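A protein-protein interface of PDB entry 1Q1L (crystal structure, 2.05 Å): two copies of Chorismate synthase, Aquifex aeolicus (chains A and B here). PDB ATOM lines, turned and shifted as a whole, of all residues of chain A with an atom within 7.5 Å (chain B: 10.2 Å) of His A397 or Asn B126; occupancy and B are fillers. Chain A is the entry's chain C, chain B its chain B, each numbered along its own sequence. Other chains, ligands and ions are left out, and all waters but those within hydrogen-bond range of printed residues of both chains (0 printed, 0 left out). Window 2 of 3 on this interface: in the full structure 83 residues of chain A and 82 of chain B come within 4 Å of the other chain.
O of Ile B123 lies within hydrogen-bond range of NE2 of His A397 (3.0 Å).
O of Lys B124 lies within hydrogen-bond range of NZ of Lys A378.
O of Gly B122 sits at hydrogen-bond distance from N of Gln B127 (2.7 Å).
OE1 of Gln B127 lies within hydrogen-bond range of ND2 of Asn B132, 3.3 Å away.
O of Tyr B125 sits at hydrogen-bond distance from NE2 of Gln B127, at 2.8 Å.
Among the printed residues, merely in contact across the chains: Phe A401 with Gly B122 (3.2 Å), Phe A401 with Ile B123 (3.3 Å), His A397 with Asn B126 (3.5 Å), Phe A401 with Asn B126 (3.6 Å), Val A398 with Ile B123 (3.7 Å) and Phe A401 with Gln B127 (3.8 Å).
Of the printed residues of chain B, Lys A378 touches Lys B124 (3.1 Å).
His A397 touches two residues of chain B.
No residue of chain B comes within 4 Å of Ser A400.
Phe A401 touches just these residues of chain B: Gly B122 (3.2 Å), Ile B123 (3.3 Å), Asn B126 (3.6 Å) and Gln B127 (3.8 Å).
Asp B118 touches none of the printed residues of chain A.
Printed residues of chain A within 4 Å of Ile B123: His A397, Val A398 and Phe A401.
Of chain A, only His A397 (3.5 Å) and Phe A401 (3.6 Å) come within 4 Å of Asn B126.
Of the printed residues of chain A, Gln B127 touches Phe A401.
The nearest residue of chain A that does not touch Asn B126 is Lys A378 (6.6 Å).
The nearest printed residue of chain B that does not touch Lys A378 is Tyr B125 (5.3 Å).
Printed residues of chain A that touch a printed residue of chain B: Lys A378, His A397, Val A398 and Phe A401.
Hydrophobic or aromatic side chains of chain A within 4 Å of the printed part of chain B: His A397, Val A398 and Phe A401.
Along chain A the printed residues that touch a printed residue of chain B span positions 378 to 401.
Among the printed residues, 8 pairs touch across the chains.
Among the printed residues, no Asp or Glu carboxylate lies within 4 Å of a Lys or Arg side-chain nitrogen of the other chain.
No position is printed for both chains.
Of the 8 pairs that touch across the chains among the printed residues, none has its exchanged pair printed and touching as well.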
ATOM      1  N   LYS A 378      11.120 -17.881  -4.082  1.00  0.00           N
ATOM      2  CA  LYS A 378      12.499 -18.358  -4.068  1.00  0.00           C
ATOM      3  C   LYS A 378      13.461 -17.496  -4.883  1.00  0.00           C
ATOM      4  O   LYS A 378      14.617 -17.313  -4.498  1.00  0.00           O
ATOM      5  CB  LYS A 378      12.540 -19.804  -4.585  1.00  0.00           C
ATOM      6  CG  LYS A 378      13.934 -20.380  -4.805  1.00  0.00           C
ATOM      7  CD  LYS A 378      14.738 -20.444  -3.512  1.00  0.00           C
ATOM      8  CE  LYS A 378      16.095 -21.091  -3.751  1.00  0.00           C
ATOM      9  NZ  LYS A 378      16.964 -21.100  -2.539  1.00  0.00           N
ATOM     10  N   PHE A 391      16.858 -18.033 -12.130  1.00  0.00           N
ATOM     11  CA  PHE A 391      16.339 -19.386 -12.282  1.00  0.00           C
ATOM     12  C   PHE A 391      17.452 -20.299 -12.788  1.00  0.00           C
ATOM     13  O   PHE A 391      17.733 -21.342 -12.197  1.00  0.00           O
ATOM     14  CB  PHE A 391      15.183 -19.406 -13.283  1.00  0.00           C
ATOM     15  CG  PHE A 391      14.543 -20.757 -13.440  1.00  0.00           C
ATOM     16  CD1 PHE A 391      13.630 -21.223 -12.501  1.00  0.00           C
ATOM     17  CD2 PHE A 391      14.863 -21.572 -14.521  1.00  0.00           C
ATOM     18  CE1 PHE A 391      13.043 -22.481 -12.636  1.00  0.00           C
ATOM     19  CE2 PHE A 391      14.282 -22.834 -14.666  1.00  0.00           C
ATOM     20  CZ  PHE A 391      13.370 -23.287 -13.722  1.00  0.00           C
ATOM     21  N   GLU A 392      18.080 -19.893 -13.887  1.00  0.00           N
ATOM     22  CA  GLU A 392      19.160 -20.663 -14.491  1.00  0.00           C
ATOM     23  C   GLU A 392      20.272 -20.898 -13.479  1.00  0.00           C
ATOM     24  O   GLU A 392      20.805 -22.002 -13.368  1.00  0.00           O
ATOM     25  CB  GLU A 392      19.701 -19.925 -15.718  1.00  0.00           C
ATOM     26  CG  GLU A 392      18.641 -19.693 -16.790  1.00  0.00           C
ATOM     27  CD  GLU A 392      19.074 -18.712 -17.861  1.00  0.00           C
ATOM     28  OE1 GLU A 392      18.270 -18.452 -18.784  1.00  0.00           O
ATOM     29  OE2 GLU A 392      20.213 -18.198 -17.782  1.00  0.00           O
ATOM     30  N   ASP A 393      20.615 -19.858 -12.732  1.00  0.00           N
ATOM     31  CA  ASP A 393      21.656 -19.966 -11.720  1.00  0.00           C
ATOM     32  C   ASP A 393      21.242 -20.953 -10.635  1.00  0.00           C
ATOM     33  O   ASP A 393      22.075 -21.689 -10.103  1.00  0.00           O
ATOM     34  CB  ASP A 393      21.927 -18.597 -11.095  1.00  0.00           C
ATOM     35  CG  ASP A 393      22.856 -17.739 -11.939  1.00  0.00           C
ATOM     36  OD1 ASP A 393      22.916 -17.943 -13.172  1.00  0.00           O
ATOM     37  OD2 ASP A 393      23.516 -16.852 -11.360  1.00  0.00           O
ATOM     38  N   TYR A 394      19.956 -20.969 -10.304  1.00  0.00           N
ATOM     39  CA  TYR A 394      19.469 -21.877  -9.274  1.00  0.00           C
ATOM     40  C   TYR A 394      19.444 -23.325  -9.763  1.00  0.00           C
ATOM     41  O   TYR A 394      19.878 -24.236  -9.056  1.00  0.00           O
ATOM     42  CB  TYR A 394      18.066 -21.476  -8.811  1.00  0.00           C
ATOM     43  CG  TYR A 394      17.502 -22.417  -7.773  1.00  0.00           C
ATOM     44  CD1 TYR A 394      18.130 -22.572  -6.539  1.00  0.00           C
ATOM     45  CD2 TYR A 394      16.368 -23.179  -8.036  1.00  0.00           C
ATOM     46  CE1 TYR A 394      17.643 -23.468  -5.592  1.00  0.00           C
ATOM     47  CE2 TYR A 394      15.870 -24.077  -7.096  1.00  0.00           C
ATOM     48  CZ  TYR A 394      16.512 -24.219  -5.876  1.00  0.00           C
ATOM     49  OH  TYR A 394      16.036 -25.112  -4.941  1.00  0.00           O
ATOM     50  N   VAL A 395      18.924 -23.530 -10.968  1.00  0.00           N
ATOM     51  CA  VAL A 395      18.846 -24.867 -11.541  1.00  0.00           C
ATOM     52  C   VAL A 395      20.236 -25.470 -11.681  1.00  0.00           C
ATOM     53  O   VAL A 395      20.438 -26.647 -11.395  1.00  0.00           O
ATOM     54  CB  VAL A 395      18.152 -24.844 -12.916  1.00  0.00           C
ATOM     55  CG1 VAL A 395      18.303 -26.190 -13.600  1.00  0.00           C
ATOM     56  CG2 VAL A 395      16.673 -24.522 -12.738  1.00  0.00           C
ATOM     57  N   ASN A 396      21.199 -24.665 -12.116  1.00  0.00           N
ATOM     58  CA  ASN A 396      22.560 -25.163 -12.250  1.00  0.00           C
ATOM     59  C   ASN A 396      23.055 -25.582 -10.875  1.00  0.00           C
ATOM     60  O   ASN A 396      23.723 -26.604 -10.732  1.00  0.00           O
ATOM     61  CB  ASN A 396      23.487 -24.087 -12.819  1.00  0.00           C
ATOM     62  CG  ASN A 396      23.181 -23.761 -14.265  1.00  0.00           C
ATOM     63  OD1 ASN A 396      22.956 -24.655 -15.080  1.00  0.00           O
ATOM     64  ND2 ASN A 396      23.185 -22.476 -14.596  1.00  0.00           N
ATOM     65  N   HIS A 397      22.720 -24.787  -9.865  1.00  0.00           N
ATOM     66  CA  HIS A 397      23.121 -25.072  -8.493  1.00  0.00           C
ATOM     67  C   HIS A 397      22.563 -26.413  -8.019  1.00  0.00           C
ATOM     68  O   HIS A 397      23.214 -27.133  -7.260  1.00  0.00           O
ATOM     69  CB  HIS A 397      22.630 -23.967  -7.555  1.00  0.00           C
ATOM     70  CG  HIS A 397      22.572 -24.383  -6.119  1.00  0.00           C
ATOM     71  ND1 HIS A 397      23.702 -24.575  -5.353  1.00  0.00           N
ATOM     72  CD2 HIS A 397      21.521 -24.700  -5.325  1.00  0.00           C
ATOM     73  CE1 HIS A 397      23.349 -24.993  -4.150  1.00  0.00           C
ATOM     74  NE2 HIS A 397      22.031 -25.077  -4.106  1.00  0.00           N
ATOM     75  N   VAL A 398      21.351 -26.733  -8.456  1.00  0.00           N
ATOM     76  CA  VAL A 398      20.715 -27.984  -8.065  1.00  0.00           C
ATOM     77  C   VAL A 398      21.430 -29.170  -8.702  1.00  0.00           C
ATOM     78  O   VAL A 398      21.846 -30.094  -8.012  1.00  0.00           O
ATOM     79  CB  VAL A 398      19.220 -28.007  -8.475  1.00  0.00           C
ATOM     80  CG1 VAL A 398      18.616 -29.373  -8.175  1.00  0.00           C
ATOM     81  CG2 VAL A 398      18.458 -26.917  -7.722  1.00  0.00           C
ATOM     82  N   LYS A 399      21.582 -29.130 -10.020  1.00  0.00           N
ATOM     83  CA  LYS A 399      22.243 -30.207 -10.746  1.00  0.00           C
ATOM     84  C   LYS A 399      23.635 -30.512 -10.206  1.00  0.00           C
ATOM     85  O   LYS A 399      23.979 -31.670  -9.985  1.00  0.00           O
ATOM     86  CB  LYS A 399      22.340 -29.857 -12.234  1.00  0.00           C
ATOM     87  CG  LYS A 399      20.991 -29.730 -12.919  1.00  0.00           C
ATOM     88  CD  LYS A 399      21.119 -29.139 -14.315  1.00  0.00           C
ATOM     89  CE  LYS A 399      19.745 -28.906 -14.933  1.00  0.00           C
ATOM     90  NZ  LYS A 399      19.820 -28.126 -16.202  1.00  0.00           N
ATOM     91  N   SER A 400      24.426 -29.468  -9.986  1.00  0.00           N
ATOM     92  CA  SER A 400      25.791 -29.629  -9.495  1.00  0.00           C
ATOM     93  C   SER A 400      25.918 -29.613  -7.976  1.00  0.00           C
ATOM     94  O   SER A 400      26.955 -29.209  -7.445  1.00  0.00           O
ATOM     95  CB  SER A 400      26.682 -28.534 -10.078  1.00  0.00           C
ATOM     96  OG  SER A 400      26.270 -27.260  -9.618  1.00  0.00           O
ATOM     97  N   PHE A 401      24.882 -30.053  -7.272  1.00  0.00           N
ATOM     98  CA  PHE A 401      24.945 -30.060  -5.816  1.00  0.00           C
ATOM     99  C   PHE A 401      25.632 -31.325  -5.301  1.00  0.00           C
ATOM    100  O   PHE A 401      25.575 -32.359  -6.003  1.00  0.00           O
ATOM    101  CB  PHE A 401      23.539 -29.957  -5.215  1.00  0.00           C
ATOM    102  CG  PHE A 401      23.535 -29.720  -3.734  1.00  0.00           C
ATOM    103  CD1 PHE A 401      24.058 -28.542  -3.208  1.00  0.00           C
ATOM    104  CD2 PHE A 401      23.034 -30.679  -2.862  1.00  0.00           C
ATOM    105  CE1 PHE A 401      24.086 -28.322  -1.832  1.00  0.00           C
ATOM    106  CE2 PHE A 401      23.055 -30.471  -1.483  1.00  0.00           C
ATOM    107  CZ  PHE A 401      23.584 -29.289  -0.967  1.00  0.00           C
ATOM    108  OXT PHE A 401      26.207 -31.271  -4.192  1.00  0.00           O
ATOM    109  N   ASP B 118      15.450 -34.305   3.344  1.00  0.00           N
ATOM    110  CA  ASP B 118      16.727 -33.783   3.813  1.00  0.00           C
ATOM    111  C   ASP B 118      17.535 -33.308   2.611  1.00  0.00           C
ATOM    112  O   ASP B 118      18.265 -32.320   2.689  1.00  0.00           O
ATOM    113  CB  ASP B 118      17.507 -34.868   4.563  1.00  0.00           C
ATOM    114  CG  ASP B 118      16.647 -35.624   5.564  1.00  0.00           C
ATOM    115  OD1 ASP B 118      15.812 -36.445   5.127  1.00  0.00           O
ATOM    116  OD2 ASP B 118      16.803 -35.394   6.784  1.00  0.00           O
ATOM    117  N   LEU B 119      17.387 -34.016   1.493  1.00  0.00           N
ATOM    118  CA  LEU B 119      18.102 -33.680   0.267  1.00  0.00           C
ATOM    119  C   LEU B 119      17.579 -32.395  -0.367  1.00  0.00           C
ATOM    120  O   LEU B 119      18.346 -31.462  -0.607  1.00  0.00           O
ATOM    121  CB  LEU B 119      17.994 -34.828  -0.743  1.00  0.00           C
ATOM    122  CG  LEU B 119      18.743 -34.629  -2.064  1.00  0.00           C
ATOM    123  CD1 LEU B 119      20.232 -34.472  -1.786  1.00  0.00           C
ATOM    124  CD2 LEU B 119      18.492 -35.811  -2.987  1.00  0.00           C
ATOM    125  N   SER B 120      16.279 -32.351  -0.643  1.00  0.00           N
ATOM    126  CA  SER B 120      15.670 -31.171  -1.248  1.00  0.00           C
ATOM    127  C   SER B 120      15.961 -29.941  -0.395  1.00  0.00           C
ATOM    128  O   SER B 120      16.264 -28.865  -0.917  1.00  0.00           O
ATOM    129  CB  SER B 120      14.159 -31.363  -1.386  1.00  0.00           C
ATOM    130  OG  SER B 120      13.864 -32.452  -2.243  1.00  0.00           O
ATOM    131  N   GLY B 121      15.866 -30.112   0.922  1.00  0.00           N
ATOM    132  CA  GLY B 121      16.133 -29.018   1.836  1.00  0.00           C
ATOM    133  C   GLY B 121      17.611 -28.684   1.829  1.00  0.00           C
ATOM    134  O   GLY B 121      17.992 -27.514   1.890  1.00  0.00           O
ATOM    135  N   GLY B 122      18.445 -29.719   1.752  1.00  0.00           N
ATOM    136  CA  GLY B 122      19.881 -29.513   1.720  1.00  0.00           C
ATOM    137  C   GLY B 122      20.283 -28.688   0.512  1.00  0.00           C
ATOM    138  O   GLY B 122      21.217 -27.891   0.577  1.00  0.00           O
ATOM    139  N   ILE B 123      19.568 -28.876  -0.596  1.00  0.00           N
ATOM    140  CA  ILE B 123      19.842 -28.140  -1.826  1.00  0.00           C
ATOM    141  C   ILE B 123      19.301 -26.713  -1.739  1.00  0.00           C
ATOM    142  O   ILE B 123      19.999 -25.750  -2.062  1.00  0.00           O
ATOM    143  CB  ILE B 123      19.193 -28.829  -3.055  1.00  0.00           C
ATOM    144  CG1 ILE B 123      19.795 -30.222  -3.255  1.00  0.00           C
ATOM    145  CG2 ILE B 123      19.399 -27.975  -4.304  1.00  0.00           C
ATOM    146  CD1 ILE B 123      19.188 -30.997  -4.413  1.00  0.00           C
ATOM    147  N   LYS B 124      18.053 -26.589  -1.300  1.00  0.00           N
ATOM    148  CA  LYS B 124      17.398 -25.291  -1.172  1.00  0.00           C
ATOM    149  C   LYS B 124      18.199 -24.297  -0.334  1.00  0.00           C
ATOM    150  O   LYS B 124      18.356 -23.140  -0.721  1.00  0.00           O
ATOM    151  CB  LYS B 124      16.006 -25.466  -0.553  1.00  0.00           C
ATOM    152  CG  LYS B 124      15.243 -24.168  -0.355  1.00  0.00           C
ATOM    153  CD  LYS B 124      13.947 -24.404   0.409  1.00  0.00           C
ATOM    154  CE  LYS B 124      13.196 -23.099   0.653  1.00  0.00           C
ATOM    155  NZ  LYS B 124      12.758 -22.450  -0.621  1.00  0.00           N
ATOM    156  N   TYR B 125      18.701 -24.754   0.811  1.00  0.00           N
ATOM    157  CA  TYR B 125      19.471 -23.904   1.718  1.00  0.00           C
ATOM    158  C   TYR B 125      20.980 -24.089   1.590  1.00  0.00           C
ATOM    159  O   TYR B 125      21.741 -23.577   2.411  1.00  0.00           O
ATOM    160  CB  TYR B 125      19.053 -24.181   3.164  1.00  0.00           C
ATOM    161  CG  TYR B 125      17.663 -23.697   3.505  1.00  0.00           C
ATOM    162  CD1 TYR B 125      17.440 -22.376   3.899  1.00  0.00           C
ATOM    163  CD2 TYR B 125      16.564 -24.554   3.411  1.00  0.00           C
ATOM    164  CE1 TYR B 125      16.156 -21.919   4.191  1.00  0.00           C
ATOM    165  CE2 TYR B 125      15.275 -24.107   3.700  1.00  0.00           C
ATOM    166  CZ  TYR B 125      15.080 -22.790   4.089  1.00  0.00           C
ATOM    167  OH  TYR B 125      13.811 -22.346   4.375  1.00  0.00           O
ATOM    168  N   ASN B 126      21.405 -24.817   0.563  1.00  0.00           N
ATOM    169  CA  ASN B 126      22.822 -25.078   0.335  1.00  0.00           C
ATOM    170  C   ASN B 126      23.496 -25.576   1.615  1.00  0.00           C
ATOM    171  O   ASN B 126      24.466 -24.986   2.095  1.00  0.00           O
ATOM    172  CB  ASN B 126      23.521 -23.809  -0.171  1.00  0.00           C
ATOM    173  CG  ASN B 126      24.988 -24.043  -0.513  1.00  0.00           C
ATOM    174  OD1 ASN B 126      25.322 -24.947  -1.280  1.00  0.00           O
ATOM    175  ND2 ASN B 126      25.867 -23.220   0.053  1.00  0.00           N
ATOM    176  N   GLN B 127      22.963 -26.663   2.166  1.00  0.00           N
ATOM    177  CA  GLN B 127      23.498 -27.265   3.381  1.00  0.00           C
ATOM    178  C   GLN B 127      24.092 -28.632   3.041  1.00  0.00           C
ATOM    179  O   GLN B 127      23.356 -29.605   2.860  1.00  0.00           O
ATOM    180  CB  GLN B 127      22.388 -27.441   4.425  1.00  0.00           C
ATOM    181  CG  GLN B 127      21.720 -26.148   4.867  1.00  0.00           C
ATOM    182  CD  GLN B 127      22.686 -25.190   5.536  1.00  0.00           C
ATOM    183  OE1 GLN B 127      23.253 -25.489   6.589  1.00  0.00           O
ATOM    184  NE2 GLN B 127      22.880 -24.028   4.922  1.00  0.00           N
ATOM    185  N   ARG B 128      25.419 -28.703   2.950  1.00  0.00           N
ATOM    186  CA  ARG B 128      26.089 -29.959   2.631  1.00  0.00           C
ATOM    187  C   ARG B 128      25.910 -30.958   3.768  1.00  0.00           C
ATOM    188  O   ARG B 128      25.866 -32.167   3.541  1.00  0.00           O
ATOM    189  CB  ARG B 128      27.579 -29.720   2.369  1.00  0.00           C
ATOM    190  CG  ARG B 128      27.855 -28.726   1.251  1.00  0.00           C
ATOM    191  CD  ARG B 128      29.331 -28.681   0.870  1.00  0.00           C
ATOM    192  NE  ARG B 128      29.693 -29.690  -0.127  1.00  0.00           N
ATOM    193  CZ  ARG B 128      29.814 -30.994   0.114  1.00  0.00           C
ATOM    194  NH1 ARG B 128      29.609 -31.479   1.331  1.00  0.00           N
ATOM    195  NH2 ARG B 128      30.143 -31.817  -0.873  1.00  0.00           N
ATOM    196  N   ASP B 129      25.814 -30.446   4.992  1.00  0.00           N
ATOM    197  CA  ASP B 129      25.605 -31.285   6.166  1.00  0.00           C
ATOM    198  C   ASP B 129      24.093 -31.421   6.327  1.00  0.00           C
ATOM    199  O   ASP B 129      23.453 -30.589   6.972  1.00  0.00           O
ATOM    200  CB  ASP B 129      26.196 -30.622   7.414  1.00  0.00           C
ATOM    201  CG  ASP B 129      26.077 -31.496   8.652  1.00  0.00           C
ATOM    202  OD1 ASP B 129      25.239 -32.423   8.656  1.00  0.00           O
ATOM    203  OD2 ASP B 129      26.817 -31.248   9.629  1.00  0.00           O
ATOM    204  N   LEU B 130      23.526 -32.469   5.734  1.00  0.00           N
ATOM    205  CA  LEU B 130      22.084 -32.697   5.786  1.00  0.00           C
ATOM    206  C   LEU B 130      21.486 -32.768   7.189  1.00  0.00           C
ATOM    207  O   LEU B 130      20.266 -32.872   7.342  1.00  0.00           O
ATOM    208  CB  LEU B 130      21.724 -33.967   5.010  1.00  0.00           C
ATOM    209  CG  LEU B 130      21.971 -33.903   3.500  1.00  0.00           C
ATOM    210  CD1 LEU B 130      21.505 -35.197   2.848  1.00  0.00           C
ATOM    211  CD2 LEU B 130      21.230 -32.711   2.908  1.00  0.00           C
ATOM    212  N   ARG B 131      22.334 -32.710   8.210  1.00  0.00           N
ATOM    213  CA  ARG B 131      21.852 -32.753   9.582  1.00  0.00           C
ATOM    214  C   ARG B 131      21.254 -31.398   9.948  1.00  0.00           C
ATOM    215  O   ARG B 131      20.485 -31.285  10.901  1.00  0.00           O
ATOM    216  CB  ARG B 131      22.993 -33.096  10.541  1.00  0.00           C
ATOM    217  CG  ARG B 131      22.544 -33.313  11.977  1.00  0.00           C
ATOM    218  CD  ARG B 131      23.654 -33.932  12.810  1.00  0.00           C
ATOM    219  NE  ARG B 131      24.216 -35.116  12.162  1.00  0.00           N
ATOM    220  CZ  ARG B 131      23.507 -36.178  11.788  1.00  0.00           C
ATOM    221  NH1 ARG B 131      22.197 -36.216  11.995  1.00  0.00           N
ATOM    222  NH2 ARG B 131      24.110 -37.204  11.200  1.00  0.00           N
ATOM    223  N   ASN B 132      21.608 -30.373   9.178  1.00  0.00           N
ATOM    224  CA  ASN B 132      21.107 -29.025   9.416  1.00  0.00           C
ATOM    225  C   ASN B 132      19.654 -28.889   8.966  1.00  0.00           C
ATOM    226  O   ASN B 132      18.950 -27.964   9.377  1.00  0.00           O
ATOM    227  CB  ASN B 132      21.971 -27.996   8.680  1.00  0.00           C
ATOM    228  CG  ASN B 132      23.420 -28.024   9.124  1.00  0.00           C
ATOM    229  OD1 ASN B 132      23.720 -27.932  10.314  1.00  0.00           O
ATOM    230  ND2 ASN B 132      24.329 -28.146   8.166  1.00  0.00           N
ATOM    231  N   ILE B 133      19.211 -29.811   8.115  1.00  0.00           N
ATOM    232  CA  ILE B 133      17.836 -29.790   7.627  1.00  0.00           C
ATOM    233  C   ILE B 133      16.974 -30.702   8.493  1.00  0.00           C
ATOM    234  O   ILE B 133      15.912 -30.296   8.970  1.00  0.00           O
ATOM    235  CB  ILE B 133      17.752 -30.257   6.151  1.00  0.00           C
ATOM    236  CG1 ILE B 133      18.567 -29.312   5.261  1.00  0.00           C
ATOM    237  CG2 ILE B 133      16.299 -30.291   5.689  1.00  0.00           C
ATOM    238  CD1 ILE B 133      18.103 -27.864   5.300  1.00  0.00           C
